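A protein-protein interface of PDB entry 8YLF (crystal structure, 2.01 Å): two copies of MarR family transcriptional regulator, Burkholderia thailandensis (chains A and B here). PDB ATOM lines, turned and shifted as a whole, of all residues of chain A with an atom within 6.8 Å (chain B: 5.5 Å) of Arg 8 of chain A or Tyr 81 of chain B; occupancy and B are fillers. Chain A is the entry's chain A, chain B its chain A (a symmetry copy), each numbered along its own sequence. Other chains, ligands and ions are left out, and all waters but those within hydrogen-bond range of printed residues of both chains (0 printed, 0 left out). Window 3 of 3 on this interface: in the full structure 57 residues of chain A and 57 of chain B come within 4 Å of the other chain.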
ATOM      1  N   MET A   6     -26.522 -15.045   3.193  1.00  0.00           N
ATOM      2  CA  MET A   6     -26.050 -14.903   4.572  1.00  0.00           C
ATOM      3  C   MET A   6     -24.839 -15.790   4.855  1.00  0.00           C
ATOM      4  O   MET A   6     -24.795 -16.944   4.427  1.00  0.00           O
ATOM      5  CB  MET A   6     -27.168 -15.239   5.566  1.00  0.00           C
ATOM      6  CG  MET A   6     -28.238 -14.164   5.722  1.00  0.00           C
ATOM      7  SD  MET A   6     -29.197 -14.349   7.252  1.00  0.00           S
ATOM      8  CE  MET A   6     -30.217 -12.871   7.193  1.00  0.00           C
ATOM      9  N   ASP A   7     -23.870 -15.254   5.598  1.00  0.00           N
ATOM     10  CA  ASP A   7     -22.676 -16.000   5.967  1.00  0.00           C
ATOM     11  C   ASP A   7     -22.912 -16.697   7.309  1.00  0.00           C
ATOM     12  O   ASP A   7     -24.030 -16.720   7.835  1.00  0.00           O
ATOM     13  CB  ASP A   7     -21.456 -15.071   5.981  1.00  0.00           C
ATOM     14  CG  ASP A   7     -21.576 -13.943   7.017  1.00  0.00           C
ATOM     15  OD1 ASP A   7     -22.696 -13.654   7.486  1.00  0.00           O
ATOM     16  OD2 ASP A   7     -20.544 -13.329   7.350  1.00  0.00           O
ATOM     17  N   ARG A   8     -21.856 -17.290   7.875  1.00  0.00           N
ATOM     18  CA  ARG A   8     -21.981 -17.972   9.161  1.00  0.00           C
ATOM     19  C   ARG A   8     -22.525 -17.032  10.225  1.00  0.00           C
ATOM     20  O   ARG A   8     -23.466 -17.373  10.953  1.00  0.00           O
ATOM     21  CB  ARG A   8     -20.622 -18.524   9.606  1.00  0.00           C
ATOM     22  CG  ARG A   8     -20.081 -19.645   8.720  1.00  0.00           C
ATOM     23  CD  ARG A   8     -18.665 -20.060   9.101  1.00  0.00           C
ATOM     24  NE  ARG A   8     -18.302 -21.293   8.410  1.00  0.00           N
ATOM     25  CZ  ARG A   8     -18.589 -22.510   8.864  1.00  0.00           C
ATOM     26  NH1 ARG A   8     -19.231 -22.655  10.021  1.00  0.00           N
ATOM     27  NH2 ARG A   8     -18.237 -23.584   8.166  1.00  0.00           N
ATOM     28  N   ALA A   9     -21.940 -15.837  10.319  1.00  0.00           N
ATOM     29  CA  ALA A   9     -22.251 -14.931  11.420  1.00  0.00           C
ATOM     30  C   ALA A   9     -23.695 -14.437  11.355  1.00  0.00           C
ATOM     31  O   ALA A   9     -24.383 -14.390  12.382  1.00  0.00           O
ATOM     32  CB  ALA A   9     -21.275 -13.759  11.415  1.00  0.00           C
ATOM     33  N   ALA A  10     -24.179 -14.070  10.167  1.00  0.00           N
ATOM     34  CA  ALA A  10     -25.550 -13.573  10.073  1.00  0.00           C
ATOM     35  C   ALA A  10     -26.555 -14.688  10.301  1.00  0.00           C
ATOM     36  O   ALA A  10     -27.604 -14.471  10.913  1.00  0.00           O
ATOM     37  CB  ALA A  10     -25.784 -12.911   8.715  1.00  0.00           C
ATOM     38  N   HIS A  11     -26.271 -15.885   9.785  1.00  0.00           N
ATOM     39  CA  HIS A  11     -27.177 -17.001  10.010  1.00  0.00           C
ATOM     40  C   HIS A  11     -27.269 -17.327  11.495  1.00  0.00           C
ATOM     41  O   HIS A  11     -28.353 -17.633  12.007  1.00  0.00           O
ATOM     42  CB  HIS A  11     -26.714 -18.217   9.210  1.00  0.00           C
ATOM     43  CG  HIS A  11     -27.516 -19.454   9.468  1.00  0.00           C
ATOM     44  ND1 HIS A  11     -28.815 -19.606   9.031  1.00  0.00           N
ATOM     45  CD2 HIS A  11     -27.203 -20.599  10.121  1.00  0.00           C
ATOM     46  CE1 HIS A  11     -29.266 -20.792   9.401  1.00  0.00           C
ATOM     47  NE2 HIS A  11     -28.307 -21.415  10.061  1.00  0.00           N
ATOM     48  N   ALA A  12     -26.141 -17.246  12.205  1.00  0.00           N
ATOM     49  CA  ALA A  12     -26.127 -17.575  13.627  1.00  0.00           C
ATOM     50  C   ALA A  12     -26.892 -16.540  14.452  1.00  0.00           C
ATOM     51  O   ALA A  12     -27.607 -16.894  15.398  1.00  0.00           O
ATOM     52  CB  ALA A  12     -24.684 -17.678  14.120  1.00  0.00           C
ATOM     53  N   VAL A  13     -26.721 -15.255  14.135  1.00  0.00           N
ATOM     54  CA  VAL A  13     -27.494 -14.215  14.808  1.00  0.00           C
ATOM     55  C   VAL A  13     -28.983 -14.424  14.564  1.00  0.00           C
ATOM     56  O   VAL A  13     -29.803 -14.288  15.481  1.00  0.00           O
ATOM     57  CB  VAL A  13     -27.026 -12.823  14.344  1.00  0.00           C
ATOM     58  CG1 VAL A  13     -28.051 -11.750  14.710  1.00  0.00           C
ATOM     59  CG2 VAL A  13     -25.669 -12.504  14.954  1.00  0.00           C
ATOM     60  N   ARG A  33     -17.305 -12.256  12.144  1.00  0.00           N
ATOM     61  CA  ARG A  33     -16.649 -12.035  10.856  1.00  0.00           C
ATOM     62  C   ARG A  33     -15.177 -11.701  11.028  1.00  0.00           C
ATOM     63  O   ARG A  33     -14.357 -12.099  10.192  1.00  0.00           O
ATOM     64  CB  ARG A  33     -17.344 -10.922  10.079  1.00  0.00           C
ATOM     65  CG  ARG A  33     -18.607 -11.385   9.415  1.00  0.00           C
ATOM     66  CD  ARG A  33     -19.297 -10.272   8.667  1.00  0.00           C
ATOM     67  NE  ARG A  33     -20.646 -10.706   8.351  1.00  0.00           N
ATOM     68  CZ  ARG A  33     -21.646  -9.892   8.056  1.00  0.00           C
ATOM     69  NH1 ARG A  33     -21.453  -8.573   8.024  1.00  0.00           N
ATOM     70  NH2 ARG A  33     -22.841 -10.410   7.801  1.00  0.00           N
ATOM     71  N   GLU A  36     -13.463 -15.104  11.811  1.00  0.00           N
ATOM     72  CA  GLU A  36     -13.512 -15.974  10.635  1.00  0.00           C
ATOM     73  C   GLU A  36     -12.619 -15.451   9.514  1.00  0.00           C
ATOM     74  O   GLU A  36     -11.934 -16.235   8.836  1.00  0.00           O
ATOM     75  CB  GLU A  36     -14.957 -16.124  10.152  1.00  0.00           C
ATOM     76  CG  GLU A  36     -15.119 -17.049   8.953  1.00  0.00           C
ATOM     77  CD  GLU A  36     -14.887 -18.512   9.300  1.00  0.00           C
ATOM     78  OE1 GLU A  36     -14.489 -18.819  10.454  1.00  0.00           O
ATOM     79  OE2 GLU A  36     -15.120 -19.362   8.410  1.00  0.00           O
ATOM     80  N   ARG A  43      -5.318 -19.443   7.099  1.00  0.00           N
ATOM     81  CA  ARG A  43      -5.305 -20.864   6.764  1.00  0.00           C
ATOM     82  C   ARG A  43      -5.212 -21.097   5.263  1.00  0.00           C
ATOM     83  O   ARG A  43      -4.457 -21.968   4.810  1.00  0.00           O
ATOM     84  CB  ARG A  43      -6.552 -21.560   7.306  1.00  0.00           C
ATOM     85  CG  ARG A  43      -6.655 -23.018   6.846  1.00  0.00           C
ATOM     86  CD  ARG A  43      -7.960 -23.667   7.277  1.00  0.00           C
ATOM     87  NE  ARG A  43      -9.089 -23.188   6.491  1.00  0.00           N
ATOM     88  CZ  ARG A  43     -10.223 -22.725   7.008  1.00  0.00           C
ATOM     89  NH1 ARG A  43     -10.402 -22.688   8.327  1.00  0.00           N
ATOM     90  NH2 ARG A  43     -11.189 -22.311   6.197  1.00  0.00           N
ATOM     91  N   ARG B  68     -28.514 -23.045  19.444  1.00  0.00           N
ATOM     92  CA  ARG B  68     -29.297 -22.165  18.592  1.00  0.00           C
ATOM     93  C   ARG B  68     -29.934 -22.906  17.436  1.00  0.00           C
ATOM     94  O   ARG B  68     -30.769 -22.324  16.737  1.00  0.00           O
ATOM     95  CB  ARG B  68     -28.454 -20.998  18.073  1.00  0.00           C
ATOM     96  CG  ARG B  68     -27.359 -21.357  17.127  1.00  0.00           C
ATOM     97  CD  ARG B  68     -26.680 -20.089  16.624  1.00  0.00           C
ATOM     98  NE  ARG B  68     -25.254 -20.309  16.439  1.00  0.00           N
ATOM     99  CZ  ARG B  68     -24.715 -20.815  15.331  1.00  0.00           C
ATOM    100  NH1 ARG B  68     -25.484 -21.134  14.293  1.00  0.00           N
ATOM    101  NH2 ARG B  68     -23.403 -20.996  15.265  1.00  0.00           N
ATOM    102  N   THR B  76     -26.113 -33.493  13.151  1.00  0.00           N
ATOM    103  CA  THR B  76     -25.031 -34.327  12.658  1.00  0.00           C
ATOM    104  C   THR B  76     -23.718 -33.555  12.781  1.00  0.00           C
ATOM    105  O   THR B  76     -23.716 -32.320  12.741  1.00  0.00           O
ATOM    106  CB  THR B  76     -25.270 -34.710  11.194  1.00  0.00           C
ATOM    107  OG1 THR B  76     -25.342 -33.513  10.407  1.00  0.00           O
ATOM    108  CG2 THR B  76     -26.568 -35.476  11.039  1.00  0.00           C
ATOM    109  N   PRO B  77     -22.580 -34.248  12.916  1.00  0.00           N
ATOM    110  CA  PRO B  77     -21.305 -33.511  12.991  1.00  0.00           C
ATOM    111  C   PRO B  77     -21.077 -32.631  11.776  1.00  0.00           C
ATOM    112  O   PRO B  77     -20.483 -31.553  11.894  1.00  0.00           O
ATOM    113  CB  PRO B  77     -20.248 -34.625  13.096  1.00  0.00           C
ATOM    114  CG  PRO B  77     -21.008 -35.878  13.439  1.00  0.00           C
ATOM    115  CD  PRO B  77     -22.377 -35.706  12.852  1.00  0.00           C
ATOM    116  N   THR B  78     -21.571 -33.045  10.610  1.00  0.00           N
ATOM    117  CA  THR B  78     -21.418 -32.213   9.419  1.00  0.00           C
ATOM    118  C   THR B  78     -22.306 -30.972   9.484  1.00  0.00           C
ATOM    119  O   THR B  78     -21.862 -29.875   9.140  1.00  0.00           O
ATOM    120  CB  THR B  78     -21.724 -33.025   8.167  1.00  0.00           C
ATOM    121  OG1 THR B  78     -20.818 -34.135   8.088  1.00  0.00           O
ATOM    122  CG2 THR B  78     -21.556 -32.160   6.917  1.00  0.00           C
ATOM    123  N   ALA B  79     -23.571 -31.128   9.887  1.00  0.00           N
ATOM    124  CA  ALA B  79     -24.412 -29.951  10.079  1.00  0.00           C
ATOM    125  C   ALA B  79     -23.814 -29.040  11.134  1.00  0.00           C
ATOM    126  O   ALA B  79     -23.900 -27.813  11.025  1.00  0.00           O
ATOM    127  CB  ALA B  79     -25.835 -30.352  10.476  1.00  0.00           C
ATOM    128  N   LEU B  80     -23.174 -29.631  12.146  1.00  0.00           N
ATOM    129  CA  LEU B  80     -22.551 -28.850  13.212  1.00  0.00           C
ATOM    130  C   LEU B  80     -21.448 -27.950  12.661  1.00  0.00           C
ATOM    131  O   LEU B  80     -21.404 -26.748  12.955  1.00  0.00           O
ATOM    132  CB  LEU B  80     -22.013 -29.809  14.279  1.00  0.00           C
ATOM    133  CG  LEU B  80     -21.446 -29.279  15.597  1.00  0.00           C
ATOM    134  CD1 LEU B  80     -22.357 -28.251  16.192  1.00  0.00           C
ATOM    135  CD2 LEU B  80     -21.261 -30.444  16.557  1.00  0.00           C
ATOM    136  N   TYR B  81     -20.566 -28.512  11.831  1.00  0.00           N
ATOM    137  CA  TYR B  81     -19.499 -27.719  11.222  1.00  0.00           C
ATOM    138  C   TYR B  81     -20.054 -26.582  10.364  1.00  0.00           C
ATOM    139  O   TYR B  81     -19.574 -25.446  10.435  1.00  0.00           O
ATOM    140  CB  TYR B  81     -18.584 -28.602  10.367  1.00  0.00           C
ATOM    141  CG  TYR B  81     -17.549 -27.780   9.627  1.00  0.00           C
ATOM    142  CD1 TYR B  81     -16.379 -27.365  10.255  1.00  0.00           C
ATOM    143  CD2 TYR B  81     -17.743 -27.405   8.301  1.00  0.00           C
ATOM    144  CE1 TYR B  81     -15.428 -26.604   9.580  1.00  0.00           C
ATOM    145  CE2 TYR B  81     -16.800 -26.646   7.621  1.00  0.00           C
ATOM    146  CZ  TYR B  81     -15.647 -26.252   8.265  1.00  0.00           C
ATOM    147  OH  TYR B  81     -14.718 -25.499   7.589  1.00  0.00           O
ATOM    148  N   ASP B  82     -21.032 -26.882   9.502  1.00  0.00           N
ATOM    149  CA  ASP B  82     -21.553 -25.843   8.615  1.00  0.00           C
ATOM    150  C   ASP B  82     -22.253 -24.720   9.383  1.00  0.00           C
ATOM    151  O   ASP B  82     -22.250 -23.574   8.927  1.00  0.00           O
ATOM    152  CB  ASP B  82     -22.505 -26.454   7.587  1.00  0.00           C
ATOM    153  CG  ASP B  82     -21.768 -27.150   6.462  1.00  0.00           C
ATOM    154  OD1 ASP B  82     -20.747 -26.608   5.995  1.00  0.00           O
ATOM    155  OD2 ASP B  82     -22.203 -28.244   6.060  1.00  0.00           O
ATOM    156  N   ALA B  83     -22.842 -25.013  10.544  1.00  0.00           N
ATOM    157  CA  ALA B  83     -23.589 -24.002  11.292  1.00  0.00           C
ATOM    158  C   ALA B  83     -22.740 -23.271  12.316  1.00  0.00           C
ATOM    159  O   ALA B  83     -23.248 -22.341  12.970  1.00  0.00           O
ATOM    160  CB  ALA B  83     -24.796 -24.637  11.987  1.00  0.00           C
ATOM    161  N   ALA B  84     -21.477 -23.666  12.476  1.00  0.00           N
ATOM    162  CA  ALA B  84     -20.633 -23.064  13.494  1.00  0.00           C
ATOM    163  C   ALA B  84     -20.389 -21.597  13.172  1.00  0.00           C
ATOM    164  O   ALA B  84     -20.459 -21.170  12.015  1.00  0.00           O
ATOM    165  CB  ALA B  84     -19.305 -23.813  13.609  1.00  0.00           C
ATOM    166  N   MET B  85     -20.140 -20.810  14.220  1.00  0.00           N
ATOM    167  CA  MET B  85     -19.742 -19.424  14.002  1.00  0.00           C
ATOM    168  C   MET B  85     -18.396 -19.346  13.289  1.00  0.00           C
ATOM    169  O   MET B  85     -18.202 -18.500  12.407  1.00  0.00           O
ATOM    170  CB  MET B  85     -19.678 -18.678  15.333  1.00  0.00           C
ATOM    171  CG  MET B  85     -19.244 -17.227  15.193  1.00  0.00           C
ATOM    172  SD  MET B  85     -20.442 -16.226  14.269  1.00  0.00           S
ATOM    173  CE  MET B  85     -21.786 -16.167  15.464  1.00  0.00           C
ATOM    174  N   ILE B  86     -17.460 -20.230  13.651  1.00  0.00           N
ATOM    175  CA  ILE B  86     -16.088 -20.218  13.153  1.00  0.00           C
ATOM    176  C   ILE B  86     -15.764 -21.569  12.522  1.00  0.00           C
ATOM    177  O   ILE B  86     -16.110 -22.621  13.069  1.00  0.00           O
ATOM    178  CB  ILE B  86     -15.080 -19.913  14.279  1.00  0.00           C
ATOM    179  CG1 ILE B  86     -15.513 -18.682  15.093  1.00  0.00           C
ATOM    180  CG2 ILE B  86     -13.682 -19.712  13.688  1.00  0.00           C
ATOM    181  CD1 ILE B  86     -15.393 -17.390  14.326  1.00  0.00           C
ATOM    182  N   SER B  87     -15.053 -21.544  11.402  1.00  0.00           N
ATOM    183  CA  SER B  87     -14.756 -22.779  10.673  1.00  0.00           C
ATOM    184  C   SER B  87     -13.417 -23.395  11.098  1.00  0.00           C
ATOM    185  O   SER B  87     -12.570 -23.731  10.267  1.00  0.00           O
ATOM    186  CB  SER B  87     -14.794 -22.507   9.174  1.00  0.00           C
ATOM    187  OG  SER B  87     -13.719 -21.680   8.769  1.00  0.00           O
ATOM    188  N   SER B  88     -13.222 -23.569  12.406  1.00  0.00           N
ATOM    189  CA  SER B  88     -12.001 -24.186  12.912  1.00  0.00           C
ATOM    190  C   SER B  88     -12.070 -25.715  12.812  1.00  0.00           C
ATOM    191  O   SER B  88     -13.145 -26.317  12.710  1.00  0.00           O
ATOM    192  CB  SER B  88     -11.733 -23.758  14.360  1.00  0.00           C
ATOM    193  OG  SER B  88     -12.923 -23.705  15.138  1.00  0.00           O
ATOM    194  N   MET B  91     -12.465 -30.833  15.318  1.00  0.00           N
ATOM    195  CA  MET B  91     -13.781 -30.872  15.947  1.00  0.00           C
ATOM    196  C   MET B  91     -14.075 -32.222  16.586  1.00  0.00           C
ATOM    197  O   MET B  91     -14.743 -32.277  17.626  1.00  0.00           O
ATOM    198  CB  MET B  91     -14.879 -30.528  14.942  1.00  0.00           C
ATOM    199  CG  MET B  91     -16.279 -30.728  15.520  1.00  0.00           C
ATOM    200  SD  MET B  91     -17.528 -29.704  14.744  1.00  0.00           S
ATOM    201  CE  MET B  91     -17.137 -28.111  15.454  1.00  0.00           C
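The guanidinium group (NH1) of Arg 8 of chain A lies within hydrogen-bond range of the backbone carbonyl oxygen (O) of Tyr 81 of chain B (2.8 Å).
The guanidinium group (NH1) of Arg 8 of chain A sits at hydrogen-bond distance from the backbone carbonyl oxygen (O) of Asp 82 of chain B, at 3.3 Å.
O of Ala 84 of chain B sits at hydrogen-bond distance from NH1 of Arg 8 of chain A.
The side-chain carboxylate (OE2) of Glu 36 of chain A is in hydrogen-bond range of the side-chain hydroxyl (OG) of Ser 87 of chain B (2.7 Å).
The backbone carbonyl oxygen (O) of Ser 87 of chain B lies within hydrogen-bond range of the guanidinium group (NH1) of Arg 43 of chain A, 3.1 Å away.
NE of Arg 8 of chain A is in salt-bridge range of OE2 of Glu 36 of chain A (3.7 Å).
The guanidinium group (NH2) of Arg 68 of chain B is in hydrogen-bond range of the backbone carbonyl oxygen (O) of Ala 83 of chain B, 2.7 Å away.
Among the printed residues, merely in contact across the chains: Arg 8 of chain A with Met 85 of chain B (3.7 Å), Arg 8 of chain A with Ser 87 of chain B (3.7 Å), Ala 9 of chain A with Met 85 of chain B (3.6 Å), Ala 12 of chain A with Arg 68 of chain B (3.4 Å), Ala 12 of chain A with Met 85 of chain B (3.5 Å) and Glu 36 of chain A with Ile 86 of chain B (3.4 Å).
Asp 7 of chain A touches none of the printed residues of chain B.
Arg 8 of chain A touches just these residues of chain B: Tyr 81 (2.8 Å), Asp 82 (3.3 Å), Ala 84 (2.8 Å), Met 85 (3.7 Å) and Ser 87 (3.7 Å).
Of the printed residues of chain B, Ala 12 of chain A touches Arg 68 (3.4 Å) and Met 85 (3.5 Å).
Of the printed residues of chain A, Arg 68 of chain B touches Ala 12.
Tyr 81 of chain B touches just one residue of chain A: Arg 8 (2.8 Å).
Of the printed residues of chain A, Met 85 of chain B touches Arg 8, Ala 9 and Ala 12.
Of the printed residues of chain A, Ile 86 of chain B touches Glu 36.
Of the printed residues of chain A, Ser 87 of chain B touches Arg 8, Glu 36 and Arg 43.
The nearest residue of chain A that does not touch Tyr 81 of chain B is Arg 43 of chain A (5.0 Å).
The nearest printed residue of chain B that does not touch Glu 36 of chain A is Met 85 of chain B (4.2 Å).
Hydrophobic or aromatic side chains of chain B that line the printed part of chain A: Tyr 81, Ala 84, Met 85 and Ile 86.
Hydrophobic or aromatic side chains of chain A within 4 Å of the printed part of chain B: Ala 9 and Ala 12.
Among the printed residues, no Asp or Glu carboxylate lies within 4 Å of a Lys or Arg side-chain nitrogen of the other chain.
No position is printed for both chains.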
